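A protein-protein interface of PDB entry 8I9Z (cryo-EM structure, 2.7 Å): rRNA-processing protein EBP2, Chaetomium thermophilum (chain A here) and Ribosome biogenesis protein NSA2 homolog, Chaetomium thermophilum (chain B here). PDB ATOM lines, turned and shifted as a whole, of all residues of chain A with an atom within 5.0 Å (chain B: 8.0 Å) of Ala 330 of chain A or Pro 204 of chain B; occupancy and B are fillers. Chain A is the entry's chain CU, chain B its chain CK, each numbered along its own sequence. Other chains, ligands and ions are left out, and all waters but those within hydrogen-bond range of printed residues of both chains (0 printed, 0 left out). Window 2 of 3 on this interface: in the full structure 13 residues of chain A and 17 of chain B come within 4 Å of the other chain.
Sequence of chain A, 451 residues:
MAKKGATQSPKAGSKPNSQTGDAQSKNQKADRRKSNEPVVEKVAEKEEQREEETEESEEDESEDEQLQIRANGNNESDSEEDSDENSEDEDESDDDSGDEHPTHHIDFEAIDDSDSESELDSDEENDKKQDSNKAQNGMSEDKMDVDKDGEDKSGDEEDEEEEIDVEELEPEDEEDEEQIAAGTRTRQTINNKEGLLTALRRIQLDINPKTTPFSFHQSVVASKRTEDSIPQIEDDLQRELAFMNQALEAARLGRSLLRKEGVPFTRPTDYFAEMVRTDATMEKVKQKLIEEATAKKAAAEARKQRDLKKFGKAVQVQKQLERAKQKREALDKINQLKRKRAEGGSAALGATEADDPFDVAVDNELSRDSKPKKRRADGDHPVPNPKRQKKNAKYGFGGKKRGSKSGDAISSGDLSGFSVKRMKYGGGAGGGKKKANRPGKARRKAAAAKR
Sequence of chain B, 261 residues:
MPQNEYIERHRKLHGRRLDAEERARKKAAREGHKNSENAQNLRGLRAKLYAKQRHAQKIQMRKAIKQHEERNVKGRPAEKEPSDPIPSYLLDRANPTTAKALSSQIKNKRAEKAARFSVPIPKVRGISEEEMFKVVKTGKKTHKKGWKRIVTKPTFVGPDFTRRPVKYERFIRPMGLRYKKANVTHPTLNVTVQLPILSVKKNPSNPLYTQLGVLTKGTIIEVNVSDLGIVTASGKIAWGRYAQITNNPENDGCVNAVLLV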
ATOM      1  N   GLN A 326     -20.835  10.630  23.963  1.00  0.00           N
ATOM      2  CA  GLN A 326     -19.865  11.714  23.860  1.00  0.00           C
ATOM      3  C   GLN A 326     -20.503  13.000  23.362  1.00  0.00           C
ATOM      4  O   GLN A 326     -20.039  14.092  23.709  1.00  0.00           O
ATOM      5  CB  GLN A 326     -18.714  11.314  22.941  1.00  0.00           C
ATOM      6  CG  GLN A 326     -17.784  10.274  23.520  1.00  0.00           C
ATOM      7  CD  GLN A 326     -17.287   9.308  22.470  1.00  0.00           C
ATOM      8  OE1 GLN A 326     -17.134   9.668  21.305  1.00  0.00           O
ATOM      9  NE2 GLN A 326     -17.032   8.069  22.876  1.00  0.00           N
ATOM     10  N   LYS A 327     -21.545  12.896  22.537  1.00  0.00           N
ATOM     11  CA  LYS A 327     -22.292  14.080  22.128  1.00  0.00           C
ATOM     12  C   LYS A 327     -22.991  14.720  23.320  1.00  0.00           C
ATOM     13  O   LYS A 327     -23.021  15.949  23.449  1.00  0.00           O
ATOM     14  CB  LYS A 327     -23.302  13.708  21.044  1.00  0.00           C
ATOM     15  CG  LYS A 327     -24.125  14.872  20.539  1.00  0.00           C
ATOM     16  CD  LYS A 327     -24.077  14.987  19.035  1.00  0.00           C
ATOM     17  CE  LYS A 327     -25.202  15.868  18.529  1.00  0.00           C
ATOM     18  NZ  LYS A 327     -26.008  15.189  17.480  1.00  0.00           N
ATOM     19  N   ARG A 328     -23.567  13.897  24.198  1.00  0.00           N
ATOM     20  CA  ARG A 328     -24.228  14.416  25.390  1.00  0.00           C
ATOM     21  C   ARG A 328     -23.233  15.088  26.326  1.00  0.00           C
ATOM     22  O   ARG A 328     -23.519  16.145  26.898  1.00  0.00           O
ATOM     23  CB  ARG A 328     -24.960  13.286  26.112  1.00  0.00           C
ATOM     24  CG  ARG A 328     -26.454  13.471  26.216  1.00  0.00           C
ATOM     25  CD  ARG A 328     -27.099  12.272  26.882  1.00  0.00           C
ATOM     26  NE  ARG A 328     -26.717  11.021  26.239  1.00  0.00           N
ATOM     27  CZ  ARG A 328     -26.634   9.852  26.859  1.00  0.00           C
ATOM     28  NH1 ARG A 328     -26.884   9.738  28.153  1.00  0.00           N
ATOM     29  NH2 ARG A 328     -26.295   8.771  26.164  1.00  0.00           N
ATOM     30  N   GLU A 329     -22.059  14.481  26.501  1.00  0.00           N
ATOM     31  CA  GLU A 329     -21.048  15.040  27.391  1.00  0.00           C
ATOM     32  C   GLU A 329     -20.483  16.343  26.841  1.00  0.00           C
ATOM     33  O   GLU A 329     -20.216  17.285  27.594  1.00  0.00           O
ATOM     34  CB  GLU A 329     -19.932  14.020  27.611  1.00  0.00           C
ATOM     35  CG  GLU A 329     -20.177  13.073  28.767  1.00  0.00           C
ATOM     36  CD  GLU A 329     -18.982  12.184  29.052  1.00  0.00           C
ATOM     37  OE1 GLU A 329     -17.944  12.709  29.509  1.00  0.00           O
ATOM     38  OE2 GLU A 329     -19.079  10.962  28.819  1.00  0.00           O
ATOM     39  N   ALA A 330     -20.280  16.405  25.524  1.00  0.00           N
ATOM     40  CA  ALA A 330     -19.767  17.624  24.911  1.00  0.00           C
ATOM     41  C   ALA A 330     -20.788  18.749  24.972  1.00  0.00           C
ATOM     42  O   ALA A 330     -20.432  19.905  25.230  1.00  0.00           O
ATOM     43  CB  ALA A 330     -19.359  17.351  23.464  1.00  0.00           C
ATOM     44  N   LEU A 331     -22.063  18.434  24.734  1.00  0.00           N
ATOM     45  CA  LEU A 331     -23.099  19.460  24.776  1.00  0.00           C
ATOM     46  C   LEU A 331     -23.336  19.951  26.199  1.00  0.00           C
ATOM     47  O   LEU A 331     -23.589  21.140  26.418  1.00  0.00           O
ATOM     48  CB  LEU A 331     -24.393  18.923  24.168  1.00  0.00           C
ATOM     49  CG  LEU A 331     -24.471  18.816  22.644  1.00  0.00           C
ATOM     50  CD1 LEU A 331     -25.909  18.640  22.212  1.00  0.00           C
ATOM     51  CD2 LEU A 331     -23.879  20.037  21.987  1.00  0.00           C
ATOM     52  N   ASP A 332     -23.263  19.047  27.180  1.00  0.00           N
ATOM     53  CA  ASP A 332     -23.448  19.443  28.572  1.00  0.00           C
ATOM     54  C   ASP A 332     -22.288  20.295  29.064  1.00  0.00           C
ATOM     55  O   ASP A 332     -22.483  21.210  29.870  1.00  0.00           O
ATOM     56  CB  ASP A 332     -23.612  18.210  29.458  1.00  0.00           C
ATOM     57  CG  ASP A 332     -24.990  17.593  29.350  1.00  0.00           C
ATOM     58  OD1 ASP A 332     -25.895  18.250  28.795  1.00  0.00           O
ATOM     59  OD2 ASP A 332     -25.171  16.450  29.820  1.00  0.00           O
ATOM     60  N   LYS A 333     -21.073  20.006  28.593  1.00  0.00           N
ATOM     61  CA  LYS A 333     -19.915  20.802  28.982  1.00  0.00           C
ATOM     62  C   LYS A 333     -19.994  22.209  28.404  1.00  0.00           C
ATOM     63  O   LYS A 333     -19.490  23.164  29.005  1.00  0.00           O
ATOM     64  CB  LYS A 333     -18.630  20.108  28.535  1.00  0.00           C
ATOM     65  CG  LYS A 333     -17.374  20.620  29.227  1.00  0.00           C
ATOM     66  CD  LYS A 333     -16.377  19.505  29.526  1.00  0.00           C
ATOM     67  CE  LYS A 333     -17.042  18.266  30.109  1.00  0.00           C
ATOM     68  NZ  LYS A 333     -17.793  18.559  31.362  1.00  0.00           N
ATOM     69  N   ILE A 334     -20.613  22.352  27.232  1.00  0.00           N
ATOM     70  CA  ILE A 334     -20.835  23.676  26.659  1.00  0.00           C
ATOM     71  C   ILE A 334     -21.836  24.458  27.501  1.00  0.00           C
ATOM     72  O   ILE A 334     -21.667  25.660  27.737  1.00  0.00           O
ATOM     73  CB  ILE A 334     -21.283  23.546  25.190  1.00  0.00           C
ATOM     74  CG1 ILE A 334     -20.135  23.016  24.335  1.00  0.00           C
ATOM     75  CG2 ILE A 334     -21.758  24.875  24.633  1.00  0.00           C
ATOM     76  CD1 ILE A 334     -20.554  22.596  22.949  1.00  0.00           C
ATOM     77  N   LYS B 201     -14.338  25.684  16.109  1.00  0.00           N
ATOM     78  CA  LYS B 201     -13.572  25.236  17.265  1.00  0.00           C
ATOM     79  C   LYS B 201     -13.951  23.838  17.731  1.00  0.00           C
ATOM     80  O   LYS B 201     -13.072  23.036  18.058  1.00  0.00           O
ATOM     81  CB  LYS B 201     -13.735  26.228  18.416  1.00  0.00           C
ATOM     82  CG  LYS B 201     -13.015  27.542  18.194  1.00  0.00           C
ATOM     83  CD  LYS B 201     -11.597  27.479  18.725  1.00  0.00           C
ATOM     84  CE  LYS B 201     -11.026  28.863  18.939  1.00  0.00           C
ATOM     85  NZ  LYS B 201     -11.058  29.659  17.684  1.00  0.00           N
ATOM     86  N   LYS B 202     -15.241  23.525  17.789  1.00  0.00           N
ATOM     87  CA  LYS B 202     -15.675  22.238  18.322  1.00  0.00           C
ATOM     88  C   LYS B 202     -16.989  21.825  17.677  1.00  0.00           C
ATOM     89  O   LYS B 202     -18.013  22.487  17.867  1.00  0.00           O
ATOM     90  CB  LYS B 202     -15.814  22.298  19.839  1.00  0.00           C
ATOM     91  CG  LYS B 202     -16.431  21.064  20.435  1.00  0.00           C
ATOM     92  CD  LYS B 202     -15.423  20.338  21.296  1.00  0.00           C
ATOM     93  CE  LYS B 202     -15.828  18.900  21.512  1.00  0.00           C
ATOM     94  NZ  LYS B 202     -15.393  18.411  22.844  1.00  0.00           N
ATOM     95  N   ASN B 203     -16.957  20.738  16.916  1.00  0.00           N
ATOM     96  CA  ASN B 203     -18.172  20.076  16.472  1.00  0.00           C
ATOM     97  C   ASN B 203     -18.471  18.923  17.418  1.00  0.00           C
ATOM     98  O   ASN B 203     -17.646  18.008  17.537  1.00  0.00           O
ATOM     99  CB  ASN B 203     -18.013  19.563  15.054  1.00  0.00           C
ATOM    100  CG  ASN B 203     -19.332  19.387  14.350  1.00  0.00           C
ATOM    101  OD1 ASN B 203     -19.725  20.218  13.537  1.00  0.00           O
ATOM    102  ND2 ASN B 203     -20.027  18.301  14.655  1.00  0.00           N
ATOM    103  N   PRO B 204     -19.610  18.915  18.097  1.00  0.00           N
ATOM    104  CA  PRO B 204     -19.831  17.917  19.148  1.00  0.00           C
ATOM    105  C   PRO B 204     -20.387  16.603  18.633  1.00  0.00           C
ATOM    106  O   PRO B 204     -20.859  15.778  19.419  1.00  0.00           O
ATOM    107  CB  PRO B 204     -20.830  18.611  20.082  1.00  0.00           C
ATOM    108  CG  PRO B 204     -21.308  19.838  19.340  1.00  0.00           C
ATOM    109  CD  PRO B 204     -20.771  19.799  17.952  1.00  0.00           C
ATOM    110  N   SER B 205     -20.340  16.393  17.320  1.00  0.00           N
ATOM    111  CA  SER B 205     -20.849  15.165  16.728  1.00  0.00           C
ATOM    112  C   SER B 205     -19.707  14.304  16.208  1.00  0.00           C
ATOM    113  O   SER B 205     -19.563  13.144  16.601  1.00  0.00           O
ATOM    114  CB  SER B 205     -21.825  15.485  15.597  1.00  0.00           C
ATOM    115  OG  SER B 205     -22.845  16.358  16.039  1.00  0.00           O
ATOM    116  N   ASN B 206     -18.897  14.865  15.336  1.00  0.00           N
ATOM    117  CA  ASN B 206     -17.762  14.187  14.729  1.00  0.00           C
ATOM    118  C   ASN B 206     -16.499  15.004  14.930  1.00  0.00           C
ATOM    119  O   ASN B 206     -16.489  16.200  14.609  1.00  0.00           O
ATOM    120  CB  ASN B 206     -18.008  13.973  13.241  1.00  0.00           C
ATOM    121  CG  ASN B 206     -17.315  12.747  12.705  1.00  0.00           C
ATOM    122  OD1 ASN B 206     -16.632  12.043  13.437  1.00  0.00           O
ATOM    123  ND2 ASN B 206     -17.487  12.486  11.415  1.00  0.00           N
ATOM    124  N   PRO B 207     -15.438  14.415  15.488  1.00  0.00           N
ATOM    125  CA  PRO B 207     -14.150  15.123  15.541  1.00  0.00           C
ATOM    126  C   PRO B 207     -13.578  15.451  14.176  1.00  0.00           C
ATOM    127  O   PRO B 207     -12.858  16.445  14.041  1.00  0.00           O
ATOM    128  CB  PRO B 207     -13.254  14.146  16.309  1.00  0.00           C
ATOM    129  CG  PRO B 207     -14.201  13.353  17.131  1.00  0.00           C
ATOM    130  CD  PRO B 207     -15.410  13.172  16.273  1.00  0.00           C
ATOM    131  N   TYR B 209     -15.360  16.413  11.677  1.00  0.00           N
ATOM    132  CA  TYR B 209     -16.096  17.589  11.228  1.00  0.00           C
ATOM    133  C   TYR B 209     -15.472  18.869  11.765  1.00  0.00           C
ATOM    134  O   TYR B 209     -15.547  19.922  11.124  1.00  0.00           O
ATOM    135  CB  TYR B 209     -17.558  17.484  11.657  1.00  0.00           C
ATOM    136  CG  TYR B 209     -18.388  16.543  10.815  1.00  0.00           C
ATOM    137  CD1 TYR B 209     -17.872  15.970   9.662  1.00  0.00           C
ATOM    138  CD2 TYR B 209     -19.695  16.243  11.168  1.00  0.00           C
ATOM    139  CE1 TYR B 209     -18.626  15.114   8.897  1.00  0.00           C
ATOM    140  CE2 TYR B 209     -20.454  15.388  10.408  1.00  0.00           C
ATOM    141  CZ  TYR B 209     -19.916  14.828   9.275  1.00  0.00           C
ATOM    142  OH  TYR B 209     -20.675  13.976   8.508  1.00  0.00           O
ATOM    143  N   THR B 210     -14.875  18.799  12.957  1.00  0.00           N
ATOM    144  CA  THR B 210     -14.137  19.936  13.494  1.00  0.00           C
ATOM    145  C   THR B 210     -12.939  20.267  12.616  1.00  0.00           C
ATOM    146  O   THR B 210     -12.687  21.437  12.307  1.00  0.00           O
ATOM    147  CB  THR B 210     -13.686  19.629  14.924  1.00  0.00           C
ATOM    148  OG1 THR B 210     -14.826  19.581  15.784  1.00  0.00           O
ATOM    149  CG2 THR B 210     -12.736  20.693  15.441  1.00  0.00           C
ATOM    150  N   VAL B 214     -17.034  21.619   9.491  1.00  0.00           N
ATOM    151  CA  VAL B 214     -18.454  21.419   9.230  1.00  0.00           C
ATOM    152  C   VAL B 214     -19.270  22.195  10.256  1.00  0.00           C
ATOM    153  O   VAL B 214     -19.012  22.116  11.462  1.00  0.00           O
ATOM    154  CB  VAL B 214     -18.795  19.920   9.249  1.00  0.00           C
ATOM    155  CG1 VAL B 214     -20.254  19.676   9.618  1.00  0.00           C
ATOM    156  CG2 VAL B 214     -18.470  19.289   7.909  1.00  0.00           C
ATOM    157  N   LEU B 215     -20.247  22.967   9.775  1.00  0.00           N
ATOM    158  CA  LEU B 215     -21.148  23.732  10.629  1.00  0.00           C
ATOM    159  C   LEU B 215     -22.390  22.891  10.908  1.00  0.00           C
ATOM    160  O   LEU B 215     -23.089  22.468   9.981  1.00  0.00           O
ATOM    161  CB  LEU B 215     -21.508  25.068   9.986  1.00  0.00           C
ATOM    162  CG  LEU B 215     -20.318  25.911   9.533  1.00  0.00           C
ATOM    163  CD1 LEU B 215     -20.755  26.976   8.559  1.00  0.00           C
ATOM    164  CD2 LEU B 215     -19.639  26.539  10.725  1.00  0.00           C
ATOM    165  N   THR B 216     -22.653  22.655  12.185  1.00  0.00           N
ATOM    166  CA  THR B 216     -23.670  21.745  12.688  1.00  0.00           C
ATOM    167  C   THR B 216     -24.322  22.415  13.894  1.00  0.00           C
ATOM    168  O   THR B 216     -23.720  23.280  14.532  1.00  0.00           O
ATOM    169  CB  THR B 216     -23.013  20.382  13.019  1.00  0.00           C
ATOM    170  OG1 THR B 216     -22.877  19.611  11.821  1.00  0.00           O
ATOM    171  CG2 THR B 216     -23.761  19.536  14.057  1.00  0.00           C
ATOM    172  N   LYS B 217     -25.586  22.085  14.161  1.00  0.00           N
ATOM    173  CA  LYS B 217     -26.249  22.577  15.359  1.00  0.00           C
ATOM    174  C   LYS B 217     -25.479  22.182  16.613  1.00  0.00           C
ATOM    175  O   LYS B 217     -25.195  21.005  16.847  1.00  0.00           O
ATOM    176  CB  LYS B 217     -27.672  22.032  15.434  1.00  0.00           C
ATOM    177  CG  LYS B 217     -28.461  22.552  16.609  1.00  0.00           C
ATOM    178  CD  LYS B 217     -29.851  21.963  16.632  1.00  0.00           C
ATOM    179  CE  LYS B 217     -30.816  22.879  17.350  1.00  0.00           C
ATOM    180  NZ  LYS B 217     -31.121  22.400  18.724  1.00  0.00           N
ATOM    181  N   GLY B 218     -25.134  23.182  17.415  1.00  0.00           N
ATOM    182  CA  GLY B 218     -24.358  22.970  18.623  1.00  0.00           C
ATOM    183  C   GLY B 218     -22.864  23.163  18.476  1.00  0.00           C
ATOM    184  O   GLY B 218     -22.127  23.003  19.455  1.00  0.00           O
ATOM    185  N   THR B 219     -22.397  23.525  17.284  1.00  0.00           N
ATOM    186  CA  THR B 219     -20.976  23.676  17.005  1.00  0.00           C
ATOM    187  C   THR B 219     -20.519  25.046  17.479  1.00  0.00           C
ATOM    188  O   THR B 219     -21.143  26.060  17.153  1.00  0.00           O
ATOM    189  CB  THR B 219     -20.684  23.494  15.509  1.00  0.00           C
ATOM    190  OG1 THR B 219     -20.611  22.098  15.207  1.00  0.00           O
ATOM    191  CG2 THR B 219     -19.376  24.147  15.107  1.00  0.00           C
ATOM    192  N   ILE B 220     -19.447  25.071  18.262  1.00  0.00           N
ATOM    193  CA  ILE B 220     -18.854  26.328  18.698  1.00  0.00           C
ATOM    194  C   ILE B 220     -17.984  26.885  17.582  1.00  0.00           C
ATOM    195  O   ILE B 220     -17.151  26.174  17.010  1.00  0.00           O
ATOM    196  CB  ILE B 220     -18.042  26.140  19.986  1.00  0.00           C
ATOM    197  CG1 ILE B 220     -18.856  25.389  21.036  1.00  0.00           C
ATOM    198  CG2 ILE B 220     -17.620  27.491  20.528  1.00  0.00           C
ATOM    199  CD1 ILE B 220     -20.152  26.059  21.405  1.00  0.00           C
ATOM    200  N   GLN B 244     -22.303  29.525  19.823  1.00  0.00           N
ATOM    201  CA  GLN B 244     -22.851  28.200  19.570  1.00  0.00           C
ATOM    202  C   GLN B 244     -23.894  28.289  18.466  1.00  0.00           C
ATOM    203  O   GLN B 244     -24.836  29.080  18.565  1.00  0.00           O
ATOM    204  CB  GLN B 244     -23.470  27.619  20.839  1.00  0.00           C
ATOM    205  CG  GLN B 244     -24.188  26.307  20.630  1.00  0.00           C
ATOM    206  CD  GLN B 244     -24.092  25.397  21.825  1.00  0.00           C
ATOM    207  OE1 GLN B 244     -23.576  24.288  21.736  1.00  0.00           O
ATOM    208  NE2 GLN B 244     -24.593  25.862  22.960  1.00  0.00           N
ATOM    209  N   ILE B 245     -23.730  27.476  17.423  1.00  0.00           N
ATOM    210  CA  ILE B 245     -24.705  27.447  16.339  1.00  0.00           C
ATOM    211  C   ILE B 245     -25.990  26.812  16.847  1.00  0.00           C
ATOM    212  O   ILE B 245     -25.995  25.668  17.317  1.00  0.00           O
ATOM    213  CB  ILE B 245     -24.142  26.701  15.126  1.00  0.00           C
ATOM    214  CG1 ILE B 245     -23.005  27.498  14.492  1.00  0.00           C
ATOM    215  CG2 ILE B 245     -25.235  26.437  14.111  1.00  0.00           C
ATOM    216  CD1 ILE B 245     -22.447  26.867  13.245  1.00  0.00           C
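The backbone NH of Lys 201 of chain B sits at hydrogen-bond distance from the backbone carbonyl oxygen of Ile 220 of chain B, at 3.0 Å. The backbone carbonyl oxygen of Lys 202 of chain B sits at hydrogen-bond distance from the backbone NH of Ile 220 of chain B (3.0 Å). N of Ser 205 of chain B lies close to ND2 of Asn 203 of chain B, 3.3 Å away. The side-chain amide oxygen of Gln 244 of chain B lies close to the backbone carbonyl oxygen of Gly 218 of chain B (3.0 Å). N of Gly 218 of chain B is in hydrogen-bond range of O of Ile 245 of chain B (2.6 Å).
Among the printed residues, merely in contact across the chains: Lys 327 of chain A with Pro 204 of chain B (3.3 Å), Ile 334 of chain A with Gln 244 of chain B (3.4 Å), Lys 327 of chain A with Ser 205 of chain B (3.5 Å), Leu 331 of chain A with Pro 204 of chain B (3.7 Å), Ile 334 of chain A with Ile 220 of chain B (3.8 Å), Ile 334 of chain A with Gly 218 of chain B (3.9 Å) and Ala 330 of chain A with Pro 204 of chain B (3.9 Å).
Printed residues of chain B within 4 Å of Lys 327 of chain A: Pro 204 and Ser 205. Ala 330 of chain A touches just one residue of chain B: Pro 204. Printed residues of chain B within 4 Å of Leu 331 of chain A: Pro 204. Pro 204 of chain B touches just these residues of chain A: Lys 327, Ala 330 and Leu 331. Of the printed residues of chain A, Gln 244 of chain B touches Ile 334. The nearest printed residue of chain A that does not touch Gly 218 of chain B is Leu 331 of chain A (4.3 Å).
Of the 18 printed residues of chain B, 5 touch a printed residue of chain A. Hydrophobic or aromatic side chains of chain B that line the printed part of chain A: Pro 204 and Ile 220. Of the 9 printed residues of chain A, 4 touch a printed residue of chain B. Printed residues of chain A that touch a printed residue of chain B: Lys 327, Ala 330, Leu 331 and Ile 334. Among the printed residues, no Asp or Glu carboxylate lies within 4 Å of a Lys or Arg side-chain nitrogen of the other chain.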
